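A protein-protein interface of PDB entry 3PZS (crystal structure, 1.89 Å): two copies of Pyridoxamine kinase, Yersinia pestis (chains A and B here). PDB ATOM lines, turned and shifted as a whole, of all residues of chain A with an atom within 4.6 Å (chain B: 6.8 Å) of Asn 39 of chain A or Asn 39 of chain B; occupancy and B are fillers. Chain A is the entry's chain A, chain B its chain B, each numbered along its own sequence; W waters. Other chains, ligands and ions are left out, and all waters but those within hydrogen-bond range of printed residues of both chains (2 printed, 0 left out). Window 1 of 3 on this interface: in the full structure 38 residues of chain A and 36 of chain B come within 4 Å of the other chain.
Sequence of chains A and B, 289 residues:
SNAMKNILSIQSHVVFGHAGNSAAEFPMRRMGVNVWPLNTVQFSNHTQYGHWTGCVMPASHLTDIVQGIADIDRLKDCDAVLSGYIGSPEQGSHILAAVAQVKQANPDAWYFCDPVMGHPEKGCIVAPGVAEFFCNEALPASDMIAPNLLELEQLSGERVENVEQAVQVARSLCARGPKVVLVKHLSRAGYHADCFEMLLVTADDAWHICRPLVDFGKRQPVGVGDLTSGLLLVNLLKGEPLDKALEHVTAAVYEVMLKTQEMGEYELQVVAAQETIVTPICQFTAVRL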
ATOM      1  N   GLN A  11      14.927 -27.475   0.756  1.00  0.00           N
ATOM      2  CA  GLN A  11      13.803 -26.903   1.485  1.00  0.00           C
ATOM      3  C   GLN A  11      14.205 -25.647   2.201  1.00  0.00           C
ATOM      4  O   GLN A  11      15.395 -25.320   2.246  1.00  0.00           O
ATOM      5  CB  GLN A  11      13.309 -27.935   2.537  1.00  0.00           C
ATOM      6  CG  GLN A  11      12.880 -29.309   1.985  1.00  0.00           C
ATOM      7  CD  GLN A  11      12.185 -30.113   3.054  1.00  0.00           C
ATOM      8  OE1 GLN A  11      11.149 -29.699   3.594  1.00  0.00           O
ATOM      9  NE2 GLN A  11      12.760 -31.250   3.410  1.00  0.00           N
ATOM     10  N   HIS A  13      15.029 -22.856   5.187  1.00  0.00           N
ATOM     11  CA  HIS A  13      15.836 -22.851   6.407  1.00  0.00           C
ATOM     12  C   HIS A  13      15.419 -21.647   7.232  1.00  0.00           C
ATOM     13  O   HIS A  13      15.313 -20.535   6.684  1.00  0.00           O
ATOM     14  CB  HIS A  13      17.357 -22.814   6.083  1.00  0.00           C
ATOM     15  CG  HIS A  13      18.231 -22.533   7.271  1.00  0.00           C
ATOM     16  ND1 HIS A  13      18.374 -23.451   8.301  1.00  0.00           N
ATOM     17  CD2 HIS A  13      18.997 -21.454   7.542  1.00  0.00           C
ATOM     18  CE1 HIS A  13      19.206 -22.892   9.164  1.00  0.00           C
ATOM     19  NE2 HIS A  13      19.611 -21.696   8.747  1.00  0.00           N
ATOM     20  N   ASN A  21      13.857 -27.630   6.055  1.00  0.00           N
ATOM     21  CA  ASN A  21      15.120 -28.276   6.367  1.00  0.00           C
ATOM     22  C   ASN A  21      15.423 -28.187   7.855  1.00  0.00           C
ATOM     23  O   ASN A  21      16.031 -29.083   8.411  1.00  0.00           O
ATOM     24  CB  ASN A  21      16.275 -27.703   5.540  1.00  0.00           C
ATOM     25  CG  ASN A  21      16.504 -28.469   4.254  1.00  0.00           C
ATOM     26  OD1 ASN A  21      15.968 -29.554   4.074  1.00  0.00           O
ATOM     27  ND2 ASN A  21      17.313 -27.914   3.363  1.00  0.00           N
ATOM     28  N   PRO A  37      21.972 -30.248   3.191  1.00  0.00           N
ATOM     29  CA  PRO A  37      20.878 -29.283   3.247  1.00  0.00           C
ATOM     30  C   PRO A  37      21.090 -28.134   2.274  1.00  0.00           C
ATOM     31  O   PRO A  37      21.877 -27.225   2.534  1.00  0.00           O
ATOM     32  CB  PRO A  37      20.891 -28.805   4.726  1.00  0.00           C
ATOM     33  CG  PRO A  37      22.031 -29.584   5.405  1.00  0.00           C
ATOM     34  CD  PRO A  37      22.948 -29.978   4.260  1.00  0.00           C
ATOM     35  N   LEU A  38      20.372 -28.182   1.154  1.00  0.00           N
ATOM     36  CA  LEU A  38      20.366 -27.118   0.154  1.00  0.00           C
ATOM     37  C   LEU A  38      19.197 -26.210   0.498  1.00  0.00           C
ATOM     38  O   LEU A  38      18.049 -26.483   0.162  1.00  0.00           O
ATOM     39  CB  LEU A  38      20.265 -27.725  -1.261  1.00  0.00           C
ATOM     40  CG  LEU A  38      20.085 -26.803  -2.501  1.00  0.00           C
ATOM     41  CD1 LEU A  38      20.946 -25.568  -2.431  1.00  0.00           C
ATOM     42  CD2 LEU A  38      20.390 -27.583  -3.790  1.00  0.00           C
ATOM     43  N   ASN A  39      19.490 -25.175   1.290  1.00  0.00           N
ATOM     44  CA  ASN A  39      18.482 -24.270   1.801  1.00  0.00           C
ATOM     45  C   ASN A  39      18.004 -23.322   0.700  1.00  0.00           C
ATOM     46  O   ASN A  39      18.821 -22.664   0.052  1.00  0.00           O
ATOM     47  CB  ASN A  39      19.051 -23.513   2.999  1.00  0.00           C
ATOM     48  CG  ASN A  39      19.489 -24.464   4.107  1.00  0.00           C
ATOM     49  OD1 ASN A  39      18.916 -25.547   4.303  1.00  0.00           O
ATOM     50  ND2 ASN A  39      20.462 -24.048   4.898  1.00  0.00           N
ATOM     51  N   THR A  40      16.678 -23.285   0.484  1.00  0.00           N
ATOM     52  CA  THR A  40      16.012 -22.458  -0.545  1.00  0.00           C
ATOM     53  C   THR A  40      15.864 -21.006  -0.082  1.00  0.00           C
ATOM     54  O   THR A  40      15.725 -20.107  -0.911  1.00  0.00           O
ATOM     55  CB  THR A  40      14.649 -23.069  -0.902  1.00  0.00           C
ATOM     56  OG1 THR A  40      13.846 -23.134   0.285  1.00  0.00           O
ATOM     57  CG2 THR A  40      14.780 -24.486  -1.480  1.00  0.00           C
ATOM     58  N   VAL A  41      15.856 -20.782   1.237  1.00  0.00           N
ATOM     59  CA  VAL A  41      15.752 -19.443   1.852  1.00  0.00           C
ATOM     60  C   VAL A  41      16.582 -19.446   3.112  1.00  0.00           C
ATOM     61  O   VAL A  41      16.898 -20.520   3.613  1.00  0.00           O
ATOM     62  CB  VAL A  41      14.259 -19.043   2.197  1.00  0.00           C
ATOM     63  CG1 VAL A  41      13.307 -19.272   1.024  1.00  0.00           C
ATOM     64  CG2 VAL A  41      13.751 -19.779   3.440  1.00  0.00           C
ATOM     65  N   GLN A  42      16.844 -18.261   3.682  1.00  0.00           N
ATOM     66  CA  GLN A  42      17.344 -18.133   5.041  1.00  0.00           C
ATOM     67  C   GLN A  42      16.473 -17.088   5.707  1.00  0.00           C
ATOM     68  O   GLN A  42      16.637 -15.911   5.416  1.00  0.00           O
ATOM     69  CB  GLN A  42      18.837 -17.802   5.159  1.00  0.00           C
ATOM     70  CG  GLN A  42      19.221 -17.683   6.650  1.00  0.00           C
ATOM     71  CD  GLN A  42      20.694 -17.847   6.851  1.00  0.00           C
ATOM     72  OE1 GLN A  42      21.522 -16.993   6.489  1.00  0.00           O
ATOM     73  NE2 GLN A  42      21.034 -18.919   7.474  1.00  0.00           N
ATOM     74  N   MET A  57      16.660 -17.553  -1.633  1.00  0.00           N
ATOM     75  CA  MET A  57      17.823 -17.692  -2.506  1.00  0.00           C
ATOM     76  C   MET A  57      17.383 -17.575  -3.972  1.00  0.00           C
ATOM     77  O   MET A  57      16.317 -18.083  -4.300  1.00  0.00           O
ATOM     78  CB  MET A  57      18.556 -19.034  -2.323  1.00  0.00           C
ATOM     79  CG  MET A  57      18.961 -19.335  -0.904  1.00  0.00           C
ATOM     80  SD  MET A  57      20.292 -18.112  -0.192  1.00  0.00           S
ATOM     81  CE  MET A  57      19.380 -17.798   1.439  1.00  0.00           C
ATOM     82  N   LEU A  62      20.231 -22.755  -6.638  1.00  0.00           N
ATOM     83  CA  LEU A  62      20.001 -24.180  -6.391  1.00  0.00           C
ATOM     84  C   LEU A  62      20.738 -25.055  -7.414  1.00  0.00           C
ATOM     85  O   LEU A  62      21.454 -25.976  -7.031  1.00  0.00           O
ATOM     86  CB  LEU A  62      18.487 -24.498  -6.385  1.00  0.00           C
ATOM     87  CG  LEU A  62      17.573 -23.626  -5.489  1.00  0.00           C
ATOM     88  CD1 LEU A  62      16.130 -24.135  -5.554  1.00  0.00           C
ATOM     89  CD2 LEU A  62      18.045 -23.609  -4.025  1.00  0.00           C
ATOM     90  N   SER B   9      24.742 -19.572  16.264  1.00  0.00           N
ATOM     91  CA  SER B   9      26.039 -19.880  15.662  1.00  0.00           C
ATOM     92  C   SER B   9      26.100 -19.221  14.269  1.00  0.00           C
ATOM     93  O   SER B   9      25.263 -19.530  13.425  1.00  0.00           O
ATOM     94  CB  SER B   9      26.240 -21.401  15.618  1.00  0.00           C
ATOM     95  OG  SER B   9      27.525 -21.672  15.088  1.00  0.00           O
ATOM     96  N   ILE B  10      27.033 -18.255  14.064  1.00  0.00           N
ATOM     97  CA  ILE B  10      27.152 -17.446  12.831  1.00  0.00           C
ATOM     98  C   ILE B  10      28.409 -17.851  12.085  1.00  0.00           C
ATOM     99  O   ILE B  10      29.504 -17.343  12.363  1.00  0.00           O
ATOM    100  CB  ILE B  10      27.139 -15.917  13.160  1.00  0.00           C
ATOM    101  CG1 ILE B  10      26.045 -15.588  14.223  1.00  0.00           C
ATOM    102  CG2 ILE B  10      26.978 -15.088  11.861  1.00  0.00           C
ATOM    103  CD1 ILE B  10      26.004 -14.100  14.721  1.00  0.00           C
ATOM    104  N   GLN B  11      28.269 -18.840  11.192  1.00  0.00           N
ATOM    105  CA  GLN B  11      29.410 -19.438  10.501  1.00  0.00           C
ATOM    106  C   GLN B  11      28.999 -19.908   9.125  1.00  0.00           C
ATOM    107  O   GLN B  11      27.813 -19.848   8.762  1.00  0.00           O
ATOM    108  CB  GLN B  11      29.958 -20.654  11.323  1.00  0.00           C
ATOM    109  CG  GLN B  11      30.395 -20.391  12.764  1.00  0.00           C
ATOM    110  CD  GLN B  11      31.032 -21.615  13.393  1.00  0.00           C
ATOM    111  OE1 GLN B  11      32.064 -22.080  12.941  1.00  0.00           O
ATOM    112  NE2 GLN B  11      30.446 -22.160  14.444  1.00  0.00           N
ATOM    113  N   SER B  12      29.979 -20.380   8.341  1.00  0.00           N
ATOM    114  CA  SER B  12      29.728 -20.831   6.968  1.00  0.00           C
ATOM    115  C   SER B  12      28.855 -22.074   6.920  1.00  0.00           C
ATOM    116  O   SER B  12      28.832 -22.845   7.890  1.00  0.00           O
ATOM    117  CB  SER B  12      31.067 -21.141   6.291  1.00  0.00           C
ATOM    118  OG  SER B  12      31.801 -19.935   6.180  1.00  0.00           O
ATOM    119  N   HIS B  13      28.167 -22.298   5.767  1.00  0.00           N
ATOM    120  CA  HIS B  13      27.361 -23.498   5.561  1.00  0.00           C
ATOM    121  C   HIS B  13      27.783 -24.129   4.244  1.00  0.00           C
ATOM    122  O   HIS B  13      27.920 -23.433   3.239  1.00  0.00           O
ATOM    123  CB  HIS B  13      25.842 -23.201   5.603  1.00  0.00           C
ATOM    124  CG  HIS B  13      24.956 -24.338   5.167  1.00  0.00           C
ATOM    125  ND1 HIS B  13      24.781 -25.473   5.954  1.00  0.00           N
ATOM    126  CD2 HIS B  13      24.199 -24.462   4.050  1.00  0.00           C
ATOM    127  CE1 HIS B  13      23.954 -26.255   5.277  1.00  0.00           C
ATOM    128  NE2 HIS B  13      23.615 -25.711   4.106  1.00  0.00           N
ATOM    129  N   VAL B  14      28.067 -25.423   4.267  1.00  0.00           N
ATOM    130  CA  VAL B  14      28.431 -26.151   3.046  1.00  0.00           C
ATOM    131  C   VAL B  14      27.333 -27.212   2.841  1.00  0.00           C
ATOM    132  O   VAL B  14      26.924 -27.844   3.813  1.00  0.00           O
ATOM    133  CB  VAL B  14      29.882 -26.727   3.061  1.00  0.00           C
ATOM    134  CG1 VAL B  14      30.913 -25.596   3.126  1.00  0.00           C
ATOM    135  CG2 VAL B  14      30.109 -27.726   4.202  1.00  0.00           C
ATOM    136  N   VAL B  15      26.793 -27.333   1.614  1.00  0.00           N
ATOM    137  CA  VAL B  15      25.685 -28.258   1.321  1.00  0.00           C
ATOM    138  C   VAL B  15      26.210 -29.694   1.378  1.00  0.00           C
ATOM    139  O   VAL B  15      25.617 -30.508   2.067  1.00  0.00           O
ATOM    140  CB  VAL B  15      24.971 -27.899  -0.002  1.00  0.00           C
ATOM    141  CG1 VAL B  15      23.901 -28.939  -0.379  1.00  0.00           C
ATOM    142  CG2 VAL B  15      24.346 -26.516   0.115  1.00  0.00           C
ATOM    143  N   ASN B  21      29.339 -24.012  10.419  1.00  0.00           N
ATOM    144  CA  ASN B  21      28.063 -24.459  10.959  1.00  0.00           C
ATOM    145  C   ASN B  21      27.734 -25.875  10.530  1.00  0.00           C
ATOM    146  O   ASN B  21      27.130 -26.598  11.303  1.00  0.00           O
ATOM    147  CB  ASN B  21      26.922 -23.519  10.553  1.00  0.00           C
ATOM    148  CG  ASN B  21      26.710 -22.402  11.547  1.00  0.00           C
ATOM    149  OD1 ASN B  21      27.203 -22.439  12.671  1.00  0.00           O
ATOM    150  ND2 ASN B  21      25.865 -21.472  11.216  1.00  0.00           N
ATOM    151  N   SER B  22      28.159 -26.295   9.333  1.00  0.00           N
ATOM    152  CA  SER B  22      27.894 -27.672   8.862  1.00  0.00           C
ATOM    153  C   SER B  22      28.724 -28.726   9.654  1.00  0.00           C
ATOM    154  O   SER B  22      28.379 -29.915   9.640  1.00  0.00           O
ATOM    155  CB  SER B  22      28.186 -27.783   7.367  1.00  0.00           C
ATOM    156  OG  SER B  22      27.492 -26.726   6.720  1.00  0.00           O
ATOM    157  N   TRP B  36      20.829 -22.145  16.645  1.00  0.00           N
ATOM    158  CA  TRP B  36      20.175 -21.251  15.691  1.00  0.00           C
ATOM    159  C   TRP B  36      21.220 -21.019  14.612  1.00  0.00           C
ATOM    160  O   TRP B  36      22.166 -20.278  14.847  1.00  0.00           O
ATOM    161  CB  TRP B  36      19.701 -19.931  16.342  1.00  0.00           C
ATOM    162  CG  TRP B  36      18.846 -20.071  17.566  1.00  0.00           C
ATOM    163  CD1 TRP B  36      18.231 -21.193  18.041  1.00  0.00           C
ATOM    164  CD2 TRP B  36      18.475 -19.008  18.444  1.00  0.00           C
ATOM    165  NE1 TRP B  36      17.513 -20.893  19.175  1.00  0.00           N
ATOM    166  CE2 TRP B  36      17.658 -19.561  19.452  1.00  0.00           C
ATOM    167  CE3 TRP B  36      18.753 -17.634  18.470  1.00  0.00           C
ATOM    168  CZ2 TRP B  36      17.127 -18.790  20.489  1.00  0.00           C
ATOM    169  CZ3 TRP B  36      18.203 -16.868  19.486  1.00  0.00           C
ATOM    170  CH2 TRP B  36      17.425 -17.452  20.493  1.00  0.00           C
ATOM    171  N   PRO B  37      21.211 -21.768  13.489  1.00  0.00           N
ATOM    172  CA  PRO B  37      22.337 -21.647  12.556  1.00  0.00           C
ATOM    173  C   PRO B  37      22.132 -20.500  11.580  1.00  0.00           C
ATOM    174  O   PRO B  37      21.346 -20.606  10.631  1.00  0.00           O
ATOM    175  CB  PRO B  37      22.387 -23.029  11.858  1.00  0.00           C
ATOM    176  CG  PRO B  37      21.176 -23.808  12.391  1.00  0.00           C
ATOM    177  CD  PRO B  37      20.258 -22.787  13.025  1.00  0.00           C
ATOM    178  N   LEU B  38      22.844 -19.386  11.844  1.00  0.00           N
ATOM    179  CA  LEU B  38      22.832 -18.194  10.986  1.00  0.00           C
ATOM    180  C   LEU B  38      24.003 -18.336  10.027  1.00  0.00           C
ATOM    181  O   LEU B  38      25.155 -18.107  10.384  1.00  0.00           O
ATOM    182  CB  LEU B  38      22.877 -16.891  11.830  1.00  0.00           C
ATOM    183  CG  LEU B  38      23.057 -15.536  11.088  1.00  0.00           C
ATOM    184  CD1 LEU B  38      22.217 -15.427   9.828  1.00  0.00           C
ATOM    185  CD2 LEU B  38      22.798 -14.368  12.028  1.00  0.00           C
ATOM    186  N   ASN B  39      23.708 -18.843   8.818  1.00  0.00           N
ATOM    187  CA  ASN B  39      24.744 -19.185   7.852  1.00  0.00           C
ATOM    188  C   ASN B  39      25.225 -17.951   7.124  1.00  0.00           C
ATOM    189  O   ASN B  39      24.411 -17.173   6.617  1.00  0.00           O
ATOM    190  CB  ASN B  39      24.232 -20.250   6.887  1.00  0.00           C
ATOM    191  CG  ASN B  39      23.745 -21.496   7.600  1.00  0.00           C
ATOM    192  OD1 ASN B  39      24.306 -21.946   8.607  1.00  0.00           O
ATOM    193  ND2 ASN B  39      22.822 -22.189   6.984  1.00  0.00           N
ATOM    194  N   THR B  40      26.549 -17.754   7.121  1.00  0.00           N
ATOM    195  CA  THR B  40      27.185 -16.578   6.513  1.00  0.00           C
ATOM    196  C   THR B  40      27.337 -16.733   5.020  1.00  0.00           C
ATOM    197  O   THR B  40      27.521 -15.738   4.322  1.00  0.00           O
ATOM    198  CB  THR B  40      28.562 -16.332   7.155  1.00  0.00           C
ATOM    199  OG1 THR B  40      29.323 -17.532   7.058  1.00  0.00           O
ATOM    200  CG2 THR B  40      28.453 -15.891   8.605  1.00  0.00           C
ATOM    201  N   VAL B  41      27.370 -17.979   4.551  1.00  0.00           N
ATOM    202  CA  VAL B  41      27.506 -18.378   3.138  1.00  0.00           C
ATOM    203  C   VAL B  41      26.686 -19.647   2.888  1.00  0.00           C
ATOM    204  O   VAL B  41      26.384 -20.389   3.822  1.00  0.00           O
ATOM    205  CB  VAL B  41      29.002 -18.637   2.715  1.00  0.00           C
ATOM    206  CG1 VAL B  41      29.957 -17.520   3.154  1.00  0.00           C
ATOM    207  CG2 VAL B  41      29.517 -19.995   3.221  1.00  0.00           C
ATOM    208  N   GLN B  42      26.434 -19.962   1.627  1.00  0.00           N
ATOM    209  CA  GLN B  42      25.918 -21.267   1.281  1.00  0.00           C
ATOM    210  C   GLN B  42      26.753 -21.701   0.088  1.00  0.00           C
ATOM    211  O   GLN B  42      26.570 -21.187  -1.012  1.00  0.00           O
ATOM    212  CB  GLN B  42      24.388 -21.335   1.052  1.00  0.00           C
ATOM    213  CG  GLN B  42      23.981 -22.732   0.496  1.00  0.00           C
ATOM    214  CD  GLN B  42      22.512 -23.032   0.620  1.00  0.00           C
ATOM    215  OE1 GLN B  42      21.652 -22.514  -0.121  1.00  0.00           O
ATOM    216  NE2 GLN B  42      22.194 -23.873   1.562  1.00  0.00           N
ATOM    217  N   MET B  57      26.516 -14.505   1.876  1.00  0.00           N
ATOM    218  CA  MET B  57      25.342 -13.701   2.232  1.00  0.00           C
ATOM    219  C   MET B  57      25.755 -12.234   2.427  1.00  0.00           C
ATOM    220  O   MET B  57      26.846 -11.998   2.953  1.00  0.00           O
ATOM    221  CB  MET B  57      24.679 -14.235   3.513  1.00  0.00           C
ATOM    222  CG  MET B  57      24.328 -15.718   3.439  1.00  0.00           C
ATOM    223  SD  MET B  57      23.134 -16.108   1.946  1.00  0.00           S
ATOM    224  CE  MET B  57      21.575 -15.252   2.678  1.00  0.00           C
ATOM    225  N   HIS B  61      22.484  -8.881   5.809  1.00  0.00           N
ATOM    226  CA  HIS B  61      21.550  -9.999   6.044  1.00  0.00           C
ATOM    227  C   HIS B  61      21.688 -10.540   7.473  1.00  0.00           C
ATOM    228  O   HIS B  61      20.681 -10.866   8.107  1.00  0.00           O
ATOM    229  CB  HIS B  61      21.807 -11.129   5.023  1.00  0.00           C
ATOM    230  CG  HIS B  61      21.016 -12.376   5.274  1.00  0.00           C
ATOM    231  ND1 HIS B  61      21.604 -13.512   5.821  1.00  0.00           N
ATOM    232  CD2 HIS B  61      19.710 -12.635   5.037  1.00  0.00           C
ATOM    233  CE1 HIS B  61      20.632 -14.410   5.912  1.00  0.00           C
ATOM    234  NE2 HIS B  61      19.483 -13.942   5.445  1.00  0.00           N
ATOM    235  N   LEU B  62      22.935 -10.636   7.991  1.00  0.00           N
ATOM    236  CA  LEU B  62      23.181 -11.199   9.325  1.00  0.00           C
ATOM    237  C   LEU B  62      22.465 -10.383  10.401  1.00  0.00           C
ATOM    238  O   LEU B  62      21.799 -10.957  11.263  1.00  0.00           O
ATOM    239  CB  LEU B  62      24.700 -11.293   9.637  1.00  0.00           C
ATOM    240  CG  LEU B  62      25.612 -11.971   8.576  1.00  0.00           C
ATOM    241  CD1 LEU B  62      27.052 -12.082   9.088  1.00  0.00           C
ATOM    242  CD2 LEU B  62      25.105 -13.371   8.221  1.00  0.00           C
HETATM  243  O   HOH W   1      21.732 -21.412   4.395  1.00  0.00           O
HETATM  244  O   HOH W   2      21.509 -25.272   7.751  1.00  0.00           O
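The backbone carbonyl oxygen of Pro 37 of chain B sits at hydrogen-bond distance from a ring nitrogen (NE2) of His 13 of chain A (2.8 Å). O of Pro 37 of chain A lies within hydrogen-bond range of NE2 of His 13 of chain B (2.8 Å). O of Asn 39 of chain A lies close to OE1 of Gln 42 of chain B, at 2.8 Å. The side-chain amide oxygen (OE1) of Gln 42 of chain A lies close to the backbone carbonyl oxygen (O) of Asn 39 of chain B, at 2.9 Å. O of Gln 42 of chain A sits at hydrogen-bond distance from NE2 of His 61 of chain B, 3.5 Å away.
Among the printed residues, pairs that only touch across the chains: His 13 of chain A with Asn 39 of chain B (3.7 Å), Pro 37 of chain A with Val 15 of chain B (3.5 Å), Pro 37 of chain A with Gln 42 of chain B (3.5 Å), Leu 38 of chain A with Val 15 of chain B (3.9 Å), Leu 38 of chain A with Gln 42 of chain B (3.9 Å), Asn 39 of chain A with His 13 of chain B (3.7 Å), Asn 39 of chain A with Asn 39 of chain B (3.7 Å), Gln 42 of chain A with Pro 37 of chain B (3.6 Å), Gln 42 of chain A with Leu 38 of chain B (3.8 Å) and Met 57 of chain A with Met 57 of chain B (3.6 Å).
Of the 11 printed residues of chain A, 6 touch a printed residue of chain B. Printed residues of chain A that touch a printed residue of chain B: His 13, Pro 37, Leu 38, Asn 39, Gln 42 and Met 57. Of the 19 printed residues of chain B, 8 touch a printed residue of chain A. Among the printed residues, no Asp or Glu carboxylate lies within 4 Å of a Lys or Arg side-chain nitrogen of the other chain.
The backbone carbonyl oxygen of Leu 38 of chain A sits at hydrogen-bond distance from the backbone NH of Gln 11 of chain A (3.3 Å). The backbone carbonyl oxygen (O) of Val 41 of chain A sits at hydrogen-bond distance from the backbone NH (N) of His 13 of chain A, 3.4 Å away. A ring nitrogen (NE2) of His 13 of chain A sits close to the side-chain amide nitrogen of Gln 42 of chain A, at 3.4 Å. The backbone carbonyl oxygen (O) of Leu 38 of chain B sits at hydrogen-bond distance from the backbone NH (N) of Gln 11 of chain B. A ring nitrogen (ND1) of His 13 of chain B sits at hydrogen-bond distance from the side-chain hydroxyl (OG) of Ser 22 of chain B (3.1 Å). The side-chain amide nitrogen (ND2) of Asn 21 of chain B lies within hydrogen-bond range of the side-chain amide oxygen (OD1) of Asn 39 of chain B (3.1 Å).
His 13 of chain A touches Pro 37 of chain B, and with the chains exchanged Pro 37 of chain A touches His 13 of chain B. His 13 of chain A touches Asn 39 of chain B, and with the chains exchanged Asn 39 of chain A touches His 13 of chain B. Asn 39 of chain A touches its own counterpart, Asn 39 of chain B. Met 57 of chain A touches its own counterpart, Met 57 of chain B. Positions printed for both chains: 11, 13, 21, 37, 38, 39, 40, 41, 42, 57 and 62. Of the 15 pairs that touch across the chains among the printed residues, 12 have their exchanged pair printed and touching as well.
Of the printed residues of chain B, His 13 of chain A touches Pro 37 and Asn 39. Of the printed residues of chain A, Val 15 of chain B touches Pro 37 (3.5 Å) and Leu 38 (3.9 Å). Asn 39 of chain B touches just these residues of chain A: His 13, Asn 39 and Gln 42. Thr 40 of chain B touches none of the printed residues of chain A. Of the printed residues of chain A, Met 57 of chain B touches Met 57 (3.6 Å). The nearest printed residue of chain A that does not touch Asn 39 of chain B is Pro 37 of chain A (6.8 Å).
Water W1 bridges the side-chain amide nitrogen of Asn 39 of chain B and the side-chain amide nitrogen of Asn 39 of chain A. Water W2 bridges the side-chain amide nitrogen of Asn 39 of chain A (3.3 Å) and the side-chain amide nitrogen of Asn 39 of chain B (3.4 Å).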
